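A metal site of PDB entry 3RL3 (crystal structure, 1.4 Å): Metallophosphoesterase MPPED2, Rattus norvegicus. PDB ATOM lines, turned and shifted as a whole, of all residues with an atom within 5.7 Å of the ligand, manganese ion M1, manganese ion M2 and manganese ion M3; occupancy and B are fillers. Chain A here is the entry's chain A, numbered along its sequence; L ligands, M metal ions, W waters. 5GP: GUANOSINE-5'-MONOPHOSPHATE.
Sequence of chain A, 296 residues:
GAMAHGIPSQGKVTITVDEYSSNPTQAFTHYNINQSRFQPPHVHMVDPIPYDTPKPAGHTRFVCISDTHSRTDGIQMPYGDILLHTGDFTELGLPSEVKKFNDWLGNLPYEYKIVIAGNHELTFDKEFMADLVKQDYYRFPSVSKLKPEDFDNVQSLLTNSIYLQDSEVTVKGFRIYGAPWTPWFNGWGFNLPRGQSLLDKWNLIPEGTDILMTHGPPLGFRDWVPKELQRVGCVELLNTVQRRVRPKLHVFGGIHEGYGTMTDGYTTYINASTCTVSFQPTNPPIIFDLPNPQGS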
ATOM      1  N   ASP A  67      -2.480 -15.867  22.127  1.00  0.00           N
ATOM      2  CA  ASP A  67      -2.118 -14.460  22.437  1.00  0.00           C
ATOM      3  C   ASP A  67      -1.910 -14.283  23.936  1.00  0.00           C
ATOM      4  O   ASP A  67      -2.440 -13.361  24.555  1.00  0.00           O
ATOM      5  CB  ASP A  67      -3.206 -13.522  21.895  1.00  0.00           C
ATOM      6  CG  ASP A  67      -3.244 -13.551  20.375  1.00  0.00           C
ATOM      7  OD1 ASP A  67      -2.472 -12.777  19.757  1.00  0.00           O
ATOM      8  OD2 ASP A  67      -4.037 -14.358  19.821  1.00  0.00           O
ATOM      9  N   HIS A  69       1.253 -13.897  25.115  1.00  0.00           N
ATOM     10  CA  HIS A  69       2.240 -12.811  25.142  1.00  0.00           C
ATOM     11  C   HIS A  69       3.133 -12.871  26.371  1.00  0.00           C
ATOM     12  O   HIS A  69       3.472 -11.838  26.949  1.00  0.00           O
ATOM     13  CB  HIS A  69       1.535 -11.459  24.996  1.00  0.00           C
ATOM     14  CG  HIS A  69       1.031 -11.194  23.611  1.00  0.00           C
ATOM     15  ND1 HIS A  69       1.860 -10.781  22.594  1.00  0.00           N
ATOM     16  CD2 HIS A  69      -0.201 -11.325  23.068  1.00  0.00           C
ATOM     17  CE1 HIS A  69       1.158 -10.646  21.481  1.00  0.00           C
ATOM     18  NE2 HIS A  69      -0.104 -10.971  21.735  1.00  0.00           N
ATOM     19  N   GLY A  87      -1.019 -19.020  18.924  1.00  0.00           N
ATOM     20  CA  GLY A  87       0.117 -18.129  18.563  1.00  0.00           C
ATOM     21  C   GLY A  87       0.235 -16.865  19.392  1.00  0.00           C
ATOM     22  O   GLY A  87      -0.630 -16.563  20.241  1.00  0.00           O
ATOM     23  N   ASP A  88       1.293 -16.094  19.148  1.00  0.00           N
ATOM     24  CA  ASP A  88       1.655 -14.981  20.012  1.00  0.00           C
ATOM     25  C   ASP A  88       1.801 -15.485  21.447  1.00  0.00           C
ATOM     26  O   ASP A  88       1.211 -14.933  22.402  1.00  0.00           O
ATOM     27  CB  ASP A  88       0.648 -13.811  19.944  1.00  0.00           C
ATOM     28  CG  ASP A  88       0.839 -12.939  18.703  1.00  0.00           C
ATOM     29  OD1 ASP A  88       1.753 -13.196  17.885  1.00  0.00           O
ATOM     30  OD2 ASP A  88       0.041 -11.995  18.546  1.00  0.00           O
ATOM     31  N   GLY A 118       2.456 -17.116  16.000  1.00  0.00           N
ATOM     32  CA  GLY A 118       1.830 -15.916  15.476  1.00  0.00           C
ATOM     33  C   GLY A 118       2.868 -14.897  15.027  1.00  0.00           C
ATOM     34  O   GLY A 118       4.069 -15.213  14.913  1.00  0.00           O
ATOM     35  N   ASN A 119       2.410 -13.673  14.811  1.00  0.00           N
ATOM     36  CA  ASN A 119       3.315 -12.623  14.271  1.00  0.00           C
ATOM     37  C   ASN A 119       4.400 -12.181  15.238  1.00  0.00           C
ATOM     38  O   ASN A 119       5.426 -11.644  14.808  1.00  0.00           O
ATOM     39  CB  ASN A 119       2.534 -11.429  13.731  1.00  0.00           C
ATOM     40  CG  ASN A 119       1.635 -10.852  14.738  1.00  0.00           C
ATOM     41  OD1 ASN A 119       0.863 -11.564  15.371  1.00  0.00           O
ATOM     42  ND2 ASN A 119       1.662  -9.541  14.876  1.00  0.00           N
ATOM     43  N   HIS A 120       4.189 -12.412  16.529  1.00  0.00           N
ATOM     44  CA  HIS A 120       5.226 -12.011  17.489  1.00  0.00           C
ATOM     45  C   HIS A 120       6.388 -13.007  17.578  1.00  0.00           C
ATOM     46  O   HIS A 120       7.431 -12.674  18.156  1.00  0.00           O
ATOM     47  CB  HIS A 120       4.641 -11.743  18.874  1.00  0.00           C
ATOM     48  CG  HIS A 120       3.933 -10.423  18.974  1.00  0.00           C
ATOM     49  ND1 HIS A 120       4.461  -9.344  19.645  1.00  0.00           N
ATOM     50  CD2 HIS A 120       2.771  -9.987  18.425  1.00  0.00           C
ATOM     51  CE1 HIS A 120       3.636  -8.318  19.554  1.00  0.00           C
ATOM     52  NE2 HIS A 120       2.612  -8.673  18.788  1.00  0.00           N
ATOM     53  N   PRO A 183      -2.818 -11.707   7.227  1.00  0.00           N
ATOM     54  CA  PRO A 183      -2.689 -10.598   6.269  1.00  0.00           C
ATOM     55  C   PRO A 183      -1.726  -9.520   6.767  1.00  0.00           C
ATOM     56  O   PRO A 183      -1.712  -9.189   7.952  1.00  0.00           O
ATOM     57  CB  PRO A 183      -4.107 -10.050   6.128  1.00  0.00           C
ATOM     58  CG  PRO A 183      -5.042 -11.040   6.773  1.00  0.00           C
ATOM     59  CD  PRO A 183      -4.212 -11.925   7.678  1.00  0.00           C
ATOM     60  N   TRP A 184      -0.913  -9.000   5.849  1.00  0.00           N
ATOM     61  CA  TRP A 184       0.131  -8.043   6.179  1.00  0.00           C
ATOM     62  C   TRP A 184      -0.428  -6.908   7.023  1.00  0.00           C
ATOM     63  O   TRP A 184      -1.440  -6.308   6.685  1.00  0.00           O
ATOM     64  CB  TRP A 184       0.742  -7.476   4.887  1.00  0.00           C
ATOM     65  CG  TRP A 184       2.140  -6.891   5.111  1.00  0.00           C
ATOM     66  CD1 TRP A 184       3.325  -7.546   4.939  1.00  0.00           C
ATOM     67  CD2 TRP A 184       2.458  -5.568   5.524  1.00  0.00           C
ATOM     68  NE1 TRP A 184       4.370  -6.688   5.237  1.00  0.00           N
ATOM     69  CE2 TRP A 184       3.865  -5.481   5.604  1.00  0.00           C
ATOM     70  CE3 TRP A 184       1.694  -4.432   5.834  1.00  0.00           C
ATOM     71  CZ2 TRP A 184       4.522  -4.298   5.973  1.00  0.00           C
ATOM     72  CZ3 TRP A 184       2.352  -3.257   6.208  1.00  0.00           C
ATOM     73  CH2 TRP A 184       3.747  -3.215   6.282  1.00  0.00           C
ATOM     74  N   PHE A 185       0.237  -6.646   8.137  1.00  0.00           N
ATOM     75  CA  PHE A 185      -0.181  -5.606   9.037  1.00  0.00           C
ATOM     76  C   PHE A 185       1.002  -4.682   9.316  1.00  0.00           C
ATOM     77  O   PHE A 185       0.984  -3.531   8.880  1.00  0.00           O
ATOM     78  CB  PHE A 185      -0.771  -6.223  10.306  1.00  0.00           C
ATOM     79  CG  PHE A 185      -1.222  -5.220  11.315  1.00  0.00           C
ATOM     80  CD1 PHE A 185      -2.068  -4.171  10.956  1.00  0.00           C
ATOM     81  CD2 PHE A 185      -0.843  -5.351  12.644  1.00  0.00           C
ATOM     82  CE1 PHE A 185      -2.479  -3.238  11.913  1.00  0.00           C
ATOM     83  CE2 PHE A 185      -1.260  -4.438  13.610  1.00  0.00           C
ATOM     84  CZ  PHE A 185      -2.082  -3.374  13.230  1.00  0.00           C
ATOM     85  N   ASN A 186       2.049  -5.189   9.956  1.00  0.00           N
ATOM     86  CA  ASN A 186       3.227  -4.368  10.321  1.00  0.00           C
ATOM     87  C   ASN A 186       4.528  -4.968   9.816  1.00  0.00           C
ATOM     88  O   ASN A 186       5.617  -4.477  10.153  1.00  0.00           O
ATOM     89  CB  ASN A 186       3.380  -4.214  11.839  1.00  0.00           C
ATOM     90  CG  ASN A 186       2.185  -3.562  12.502  1.00  0.00           C
ATOM     91  OD1 ASN A 186       1.661  -2.550  12.038  1.00  0.00           O
ATOM     92  ND2 ASN A 186       1.769  -4.129  13.638  1.00  0.00           N
ATOM     93  N   ARG A 194      -2.679  -9.884   1.244  1.00  0.00           N
ATOM     94  CA  ARG A 194      -3.938 -10.502   0.903  1.00  0.00           C
ATOM     95  C   ARG A 194      -3.949 -11.026  -0.524  1.00  0.00           C
ATOM     96  O   ARG A 194      -3.261 -10.510  -1.413  1.00  0.00           O
ATOM     97  CB  ARG A 194      -5.073  -9.499   1.121  1.00  0.00           C
ATOM     98  CG  ARG A 194      -5.303  -9.185   2.588  1.00  0.00           C
ATOM     99  CD  ARG A 194      -6.442  -8.177   2.814  1.00  0.00           C
ATOM    100  NE  ARG A 194      -6.466  -7.731   4.213  1.00  0.00           N
ATOM    101  CZ  ARG A 194      -7.117  -8.359   5.181  1.00  0.00           C
ATOM    102  NH1 ARG A 194      -7.807  -9.462   4.929  1.00  0.00           N
ATOM    103  NH2 ARG A 194      -7.071  -7.873   6.427  1.00  0.00           N
ATOM    104  N   HIS A 215      -3.422 -18.205  13.162  1.00  0.00           N
ATOM    105  CA  HIS A 215      -3.196 -17.180  14.166  1.00  0.00           C
ATOM    106  C   HIS A 215      -4.316 -16.157  14.154  1.00  0.00           C
ATOM    107  O   HIS A 215      -4.745 -15.693  15.199  1.00  0.00           O
ATOM    108  CB  HIS A 215      -1.837 -16.515  14.035  1.00  0.00           C
ATOM    109  CG  HIS A 215      -1.634 -15.423  15.050  1.00  0.00           C
ATOM    110  ND1 HIS A 215      -1.778 -15.652  16.410  1.00  0.00           N
ATOM    111  CD2 HIS A 215      -1.325 -14.108  14.913  1.00  0.00           C
ATOM    112  CE1 HIS A 215      -1.582 -14.518  17.060  1.00  0.00           C
ATOM    113  NE2 HIS A 215      -1.305 -13.559  16.183  1.00  0.00           N
ATOM    114  N   VAL A 225     -12.285  -4.891  14.326  1.00  0.00           N
ATOM    115  CA  VAL A 225     -11.302  -4.060  15.028  1.00  0.00           C
ATOM    116  C   VAL A 225     -11.979  -2.710  15.330  1.00  0.00           C
ATOM    117  O   VAL A 225     -12.101  -1.876  14.432  1.00  0.00           O
ATOM    118  CB  VAL A 225      -9.996  -3.889  14.201  1.00  0.00           C
ATOM    119  CG1 VAL A 225      -8.979  -3.028  14.934  1.00  0.00           C
ATOM    120  CG2 VAL A 225      -9.385  -5.255  13.879  1.00  0.00           C
ATOM    121  N   LYS A 227     -11.203   0.060  16.840  1.00  0.00           N
ATOM    122  CA  LYS A 227     -10.463   1.307  16.661  1.00  0.00           C
ATOM    123  C   LYS A 227     -10.454   1.742  15.208  1.00  0.00           C
ATOM    124  O   LYS A 227     -10.430   2.937  14.921  1.00  0.00           O
ATOM    125  CB  LYS A 227      -9.041   1.235  17.236  1.00  0.00           C
ATOM    126  CG  LYS A 227      -8.087   0.320  16.525  1.00  0.00           C
ATOM    127  CD  LYS A 227      -6.977  -0.127  17.464  1.00  0.00           C
ATOM    128  CE  LYS A 227      -6.417  -1.474  17.030  1.00  0.00           C
ATOM    129  NZ  LYS A 227      -5.484  -2.037  18.032  1.00  0.00           N
ATOM    130  N   GLU A 228     -10.478   0.763  14.293  1.00  0.00           N
ATOM    131  CA  GLU A 228     -10.429   1.047  12.865  1.00  0.00           C
ATOM    132  C   GLU A 228     -11.801   1.028  12.204  1.00  0.00           C
ATOM    133  O   GLU A 228     -11.929   1.436  11.041  1.00  0.00           O
ATOM    134  CB  GLU A 228      -9.521   0.046  12.137  1.00  0.00           C
ATOM    135  CG  GLU A 228      -8.050   0.217  12.447  1.00  0.00           C
ATOM    136  CD  GLU A 228      -7.511   1.532  11.923  1.00  0.00           C
ATOM    137  OE1 GLU A 228      -7.124   1.610  10.734  1.00  0.00           O
ATOM    138  OE2 GLU A 228      -7.485   2.505  12.710  1.00  0.00           O
ATOM    139  N   GLN A 230     -13.324  -1.580  11.170  1.00  0.00           N
ATOM    140  CA  GLN A 230     -13.072  -2.418  10.012  1.00  0.00           C
ATOM    141  C   GLN A 230     -13.073  -3.886  10.402  1.00  0.00           C
ATOM    142  O   GLN A 230     -12.654  -4.258  11.516  1.00  0.00           O
ATOM    143  CB  GLN A 230     -11.726  -2.082   9.377  1.00  0.00           C
ATOM    144  CG  GLN A 230     -11.731  -0.801   8.535  1.00  0.00           C
ATOM    145  CD  GLN A 230     -10.560  -0.715   7.579  1.00  0.00           C
ATOM    146  OE1 GLN A 230      -9.505  -1.304   7.818  1.00  0.00           O
ATOM    147  NE2 GLN A 230     -10.747   0.030   6.493  1.00  0.00           N
ATOM    148  N   VAL A 232     -11.160  -7.360   9.522  1.00  0.00           N
ATOM    149  CA  VAL A 232      -9.803  -7.597   9.031  1.00  0.00           C
ATOM    150  C   VAL A 232      -9.490  -9.074   8.746  1.00  0.00           C
ATOM    151  O   VAL A 232      -8.349  -9.409   8.403  1.00  0.00           O
ATOM    152  CB  VAL A 232      -8.717  -7.025   9.985  1.00  0.00           C
ATOM    153  CG1 VAL A 232      -8.906  -5.506  10.191  1.00  0.00           C
ATOM    154  CG2 VAL A 232      -8.727  -7.744  11.330  1.00  0.00           C
ATOM    155  N   GLY A 254      -5.384 -13.528  17.343  1.00  0.00           N
ATOM    156  CA  GLY A 254      -4.935 -12.468  16.435  1.00  0.00           C
ATOM    157  C   GLY A 254      -5.550 -11.130  16.771  1.00  0.00           C
ATOM    158  O   GLY A 254      -4.841 -10.184  17.146  1.00  0.00           O
ATOM    159  N   ILE A 255      -6.864 -11.062  16.617  1.00  0.00           N
ATOM    160  CA  ILE A 255      -7.627  -9.854  16.990  1.00  0.00           C
ATOM    161  C   ILE A 255      -8.105 -10.040  18.416  1.00  0.00           C
ATOM    162  O   ILE A 255      -9.107 -10.735  18.662  1.00  0.00           O
ATOM    163  CB  ILE A 255      -8.778  -9.621  15.996  1.00  0.00           C
ATOM    164  CG1 ILE A 255      -8.218  -9.528  14.560  1.00  0.00           C
ATOM    165  CG2 ILE A 255      -9.588  -8.355  16.357  1.00  0.00           C
ATOM    166  CD1 ILE A 255      -7.076  -8.477  14.360  1.00  0.00           C
ATOM    167  N   HIS A 256      -7.364  -9.470  19.362  1.00  0.00           N
ATOM    168  CA  HIS A 256      -7.642  -9.737  20.792  1.00  0.00           C
ATOM    169  C   HIS A 256      -9.067  -9.351  21.147  1.00  0.00           C
ATOM    170  O   HIS A 256      -9.736 -10.053  21.935  1.00  0.00           O
ATOM    171  CB  HIS A 256      -6.674  -8.981  21.705  1.00  0.00           C
ATOM    172  CG  HIS A 256      -5.231  -9.350  21.538  1.00  0.00           C
ATOM    173  ND1 HIS A 256      -4.247  -8.820  22.346  1.00  0.00           N
ATOM    174  CD2 HIS A 256      -4.586 -10.181  20.670  1.00  0.00           C
ATOM    175  CE1 HIS A 256      -3.065  -9.276  21.983  1.00  0.00           C
ATOM    176  NE2 HIS A 256      -3.236 -10.111  20.964  1.00  0.00           N
ATOM    177  N   GLU A 257      -9.514  -8.243  20.569  1.00  0.00           N
ATOM    178  CA  GLU A 257     -10.878  -7.697  20.798  1.00  0.00           C
ATOM    179  C   GLU A 257     -11.991  -8.662  20.443  1.00  0.00           C
ATOM    180  O   GLU A 257     -13.142  -8.506  20.888  1.00  0.00           O
ATOM    181  CB  GLU A 257     -11.097  -6.402  19.984  1.00  0.00           C
ATOM    182  CG  GLU A 257     -10.107  -5.291  20.197  1.00  0.00           C
ATOM    183  CD  GLU A 257      -8.966  -5.361  19.210  1.00  0.00           C
ATOM    184  OE1 GLU A 257      -8.218  -6.342  19.264  1.00  0.00           O
ATOM    185  OE2 GLU A 257      -8.752  -4.443  18.398  1.00  0.00           O
ATOM    186  N   VAL A 277      -7.012  -6.167  24.262  1.00  0.00           N
ATOM    187  CA  VAL A 277      -6.288  -5.268  23.349  1.00  0.00           C
ATOM    188  C   VAL A 277      -5.214  -4.444  24.101  1.00  0.00           C
ATOM    189  O   VAL A 277      -4.265  -3.948  23.486  1.00  0.00           O
ATOM    190  CB  VAL A 277      -7.275  -4.349  22.549  1.00  0.00           C
ATOM    191  CG1 VAL A 277      -7.929  -3.331  23.485  1.00  0.00           C
ATOM    192  CG2 VAL A 277      -6.551  -3.665  21.367  1.00  0.00           C
ATOM    193  N   PHE A 279      -3.399  -5.893  26.417  1.00  0.00           N
ATOM    194  CA  PHE A 279      -2.426  -6.916  26.776  1.00  0.00           C
ATOM    195  C   PHE A 279      -2.555  -7.427  28.211  1.00  0.00           C
ATOM    196  O   PHE A 279      -1.573  -7.852  28.825  1.00  0.00           O
ATOM    197  CB  PHE A 279      -0.991  -6.464  26.422  1.00  0.00           C
ATOM    198  CG  PHE A 279      -0.684  -6.560  24.938  1.00  0.00           C
ATOM    199  CD1 PHE A 279      -1.219  -5.644  24.044  1.00  0.00           C
ATOM    200  CD2 PHE A 279       0.128  -7.584  24.443  1.00  0.00           C
ATOM    201  CE1 PHE A 279      -0.933  -5.746  22.659  1.00  0.00           C
ATOM    202  CE2 PHE A 279       0.415  -7.681  23.081  1.00  0.00           C
ATOM    203  CZ  PHE A 279      -0.120  -6.764  22.188  1.00  0.00           C
HETATM  204  P   5GP L   1      -0.626  -8.395  17.944  1.00  0.00           P
HETATM  205  O1P 5GP L   1      -0.476  -9.333  16.782  1.00  0.00           O
HETATM  206  O2P 5GP L   1      -0.580  -9.118  19.368  1.00  0.00           O
HETATM  207  O3P 5GP L   1       0.507  -7.312  17.893  1.00  0.00           O
HETATM  208  O5' 5GP L   1      -2.041  -7.637  17.810  1.00  0.00           O
HETATM  209  C5' 5GP L   1      -2.551  -6.859  18.892  1.00  0.00           C
HETATM  210  C4' 5GP L   1      -3.748  -6.004  18.371  1.00  0.00           C
HETATM  211  O4' 5GP L   1      -3.327  -5.298  17.166  1.00  0.00           O
HETATM  212  C3' 5GP L   1      -4.974  -6.770  17.873  1.00  0.00           C
HETATM  213  O3' 5GP L   1      -5.775  -7.130  18.969  1.00  0.00           O
HETATM  214  C2' 5GP L   1      -5.657  -5.709  17.010  1.00  0.00           C
HETATM  215  O2' 5GP L   1      -6.219  -4.634  17.809  1.00  0.00           O
HETATM  216  C1' 5GP L   1      -4.448  -5.159  16.276  1.00  0.00           C
HETATM  217  N9  5GP L   1      -4.276  -5.931  15.025  1.00  0.00           N
HETATM  218  C8  5GP L   1      -3.698  -7.124  14.859  1.00  0.00           C
HETATM  219  N7  5GP L   1      -3.761  -7.469  13.569  1.00  0.00           N
HETATM  220  C5  5GP L   1      -4.386  -6.493  12.915  1.00  0.00           C
HETATM  221  C6  5GP L   1      -4.755  -6.285  11.585  1.00  0.00           C
HETATM  222  O6  5GP L   1      -4.475  -7.104  10.715  1.00  0.00           O
HETATM  223  N1  5GP L   1      -5.420  -5.112  11.239  1.00  0.00           N
HETATM  224  C2  5GP L   1      -5.712  -4.171  12.242  1.00  0.00           C
HETATM  225  N2  5GP L   1      -6.337  -3.037  11.934  1.00  0.00           N
HETATM  226  N3  5GP L   1      -5.356  -4.402  13.510  1.00  0.00           N
HETATM  227  C4  5GP L   1      -4.714  -5.521  13.849  1.00  0.00           C
HETATM  228 MN    MN M   1      -0.822 -11.380  16.527  1.00  0.00          MN
HETATM  229 MN    MN M   2      -1.413 -10.966  19.921  1.00  0.00          MN
HETATM  230 MN    MN M   3       0.866  -5.335  17.289  1.00  0.00          MN
HETATM  231  O   HOH W   1       0.910  -4.796  18.929  1.00  0.00           O
HETATM  232  O   HOH W   2      -4.334 -10.689  13.685  1.00  0.00           O
HETATM  233  O   HOH W   3      -2.287  -2.126  16.618  1.00  0.00           O
HETATM  234  O   HOH W   4       2.123  -6.423  15.567  1.00  0.00           O
HETATM  235  O   HOH W   5      -1.794 -10.941  14.691  1.00  0.00           O
HETATM  236  O   HOH W   6      -4.227  -6.586   7.731  1.00  0.00           O
HETATM  237  O   HOH W   7      -2.724  -9.321  10.446  1.00  0.00           O
HETATM  238  O   HOH W   8      -2.505 -11.056  17.851  1.00  0.00           O
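Water W1 is bound to manganese ion M3, at 1.7 Å.
Manganese ion M3 is bound by O3P of the ligand, 2.1 Å away.
Manganese ion M3 is bound by water W4, 2.4 Å away.
Manganese ion M1 is bound by OD1 of Asn 119, at 2.1 Å.
O1P of the ligand binds manganese ion M1 (2.1 Å).
Water W5 is bound to manganese ion M1 (2.1 Å).
Manganese ion M1 is bound by water W8, 2.2 Å away.
A ring nitrogen (NE2) of His 215 is bound to manganese ion M1, at 2.3 Å.
The side-chain carboxylate (OD2) of Asp 88 is bound to manganese ion M1, at 2.3 Å.
Water W8 bridges O of Gly 254 (2.6 Å) and O5' of the ligand (3.5 Å).
Water W4 lies within hydrogen-bond range of the side-chain amide nitrogen (ND2) of Asn 186 (3.0 Å) and the side-chain amide nitrogen (ND2) of Asn 119 (3.2 Å).
Water W7 lies within hydrogen-bond range of O of Pro 183 (2.7 Å) and O6 of the ligand (2.8 Å).
Water W6 lies within hydrogen-bond range of O of Trp 184 (3.0 Å), O6 of the ligand (3.0 Å) and NH2 of Arg 194 (3.4 Å).
Water W3 bridges an oxygen (O4') of the ligand (3.4 Å) and the side-chain amino group (NZ) of Lys 227 (3.5 Å).
CE1 of Phe 185 touches C2 of the ligand, at 3.4 Å.
Val 225 touches the ligand.
CG of Glu 228 touches N2 of the ligand (3.7 Å).
Val 232 touches the ligand.
Gly 254 touches the ligand.
Ile 255 touches the ligand.
Val 277 touches the ligand (CG2 to O2', 3.7 Å).
CZ of Phe 279 touches O2P of the ligand, 3.7 Å away.
Hydrophobic or aromatic side chains within 4 Å of the ligand: His 69, His 120, Phe 185, Val 225, Val 232, Ile 255, His 256, Val 277 and Phe 279.
Within 4 Å of the ligand: His 69, Asp 88, Asn 119, His 120, Phe 185, Val 225, Lys 227, Glu 228, Val 232, Gly 254, Ile 255, His 256, Glu 257, Val 277 and Phe 279.
Of the 24 residues printed, 4 come within 4 Å of manganese ion M2.
The nearest printed residue that does not touch manganese ion M2 is Gly 254 (4.5 Å).
Merely in contact with manganese ion M3: Asn 186 (3.9 Å).
The nearest printed residue that does not touch manganese ion M3 is His 120 (4.1 Å).
The side-chain carboxylate (OD1) of Asp 88 sits at hydrogen-bond distance from the backbone NH (N) of His 120 (2.9 Å).
The backbone carbonyl oxygen (O) of Val 232 is in hydrogen-bond range of the guanidinium group (NH2) of Arg 194, 2.8 Å away.
The backbone carbonyl oxygen (O) of Gln 230 sits at hydrogen-bond distance from the backbone NH (N) of Val 225 (2.9 Å).
The backbone carbonyl oxygen (O) of His 215 sits at hydrogen-bond distance from the backbone NH (N) of Gly 254 (3.1 Å).
The side-chain carboxylate of Asp 67 sits at hydrogen-bond distance from the backbone NH of Gly 254 (2.9 Å).
The backbone NH (N) of Asp 67 lies within hydrogen-bond range of the backbone carbonyl oxygen (O) of Gly 87, 2.7 Å away.
Within 4 Å of manganese ion M1: Asp 67, Asp 88, Asn 119 and His 215.
Manganese ion M2 is bound by O2P of the ligand (2.1 Å).
Manganese ion M2 is bound by OD1 of Asp 67, at 2.1 Å.
Manganese ion M2 is bound by NE2 of His 69, at 2.2 Å.
Manganese ion M2 is bound by OD2 of Asp 88, 2.3 Å away.
NE2 of His 256 is bound to manganese ion M2 (2.3 Å).
Water W8 is bound to manganese ion M2, at 2.3 Å.
A ring nitrogen (NE2) of His 120 lies close to an oxygen (O3P) of the ligand.
The side-chain amino group (NZ) of Lys 227 is in hydrogen-bond range of an oxygen (O2') of the ligand.
The backbone NH (N) of His 256 lies within hydrogen-bond range of an oxygen (O3') of the ligand, 2.9 Å away.
OE1 of Glu 257 lies within hydrogen-bond range of O3' of the ligand (2.6 Å).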
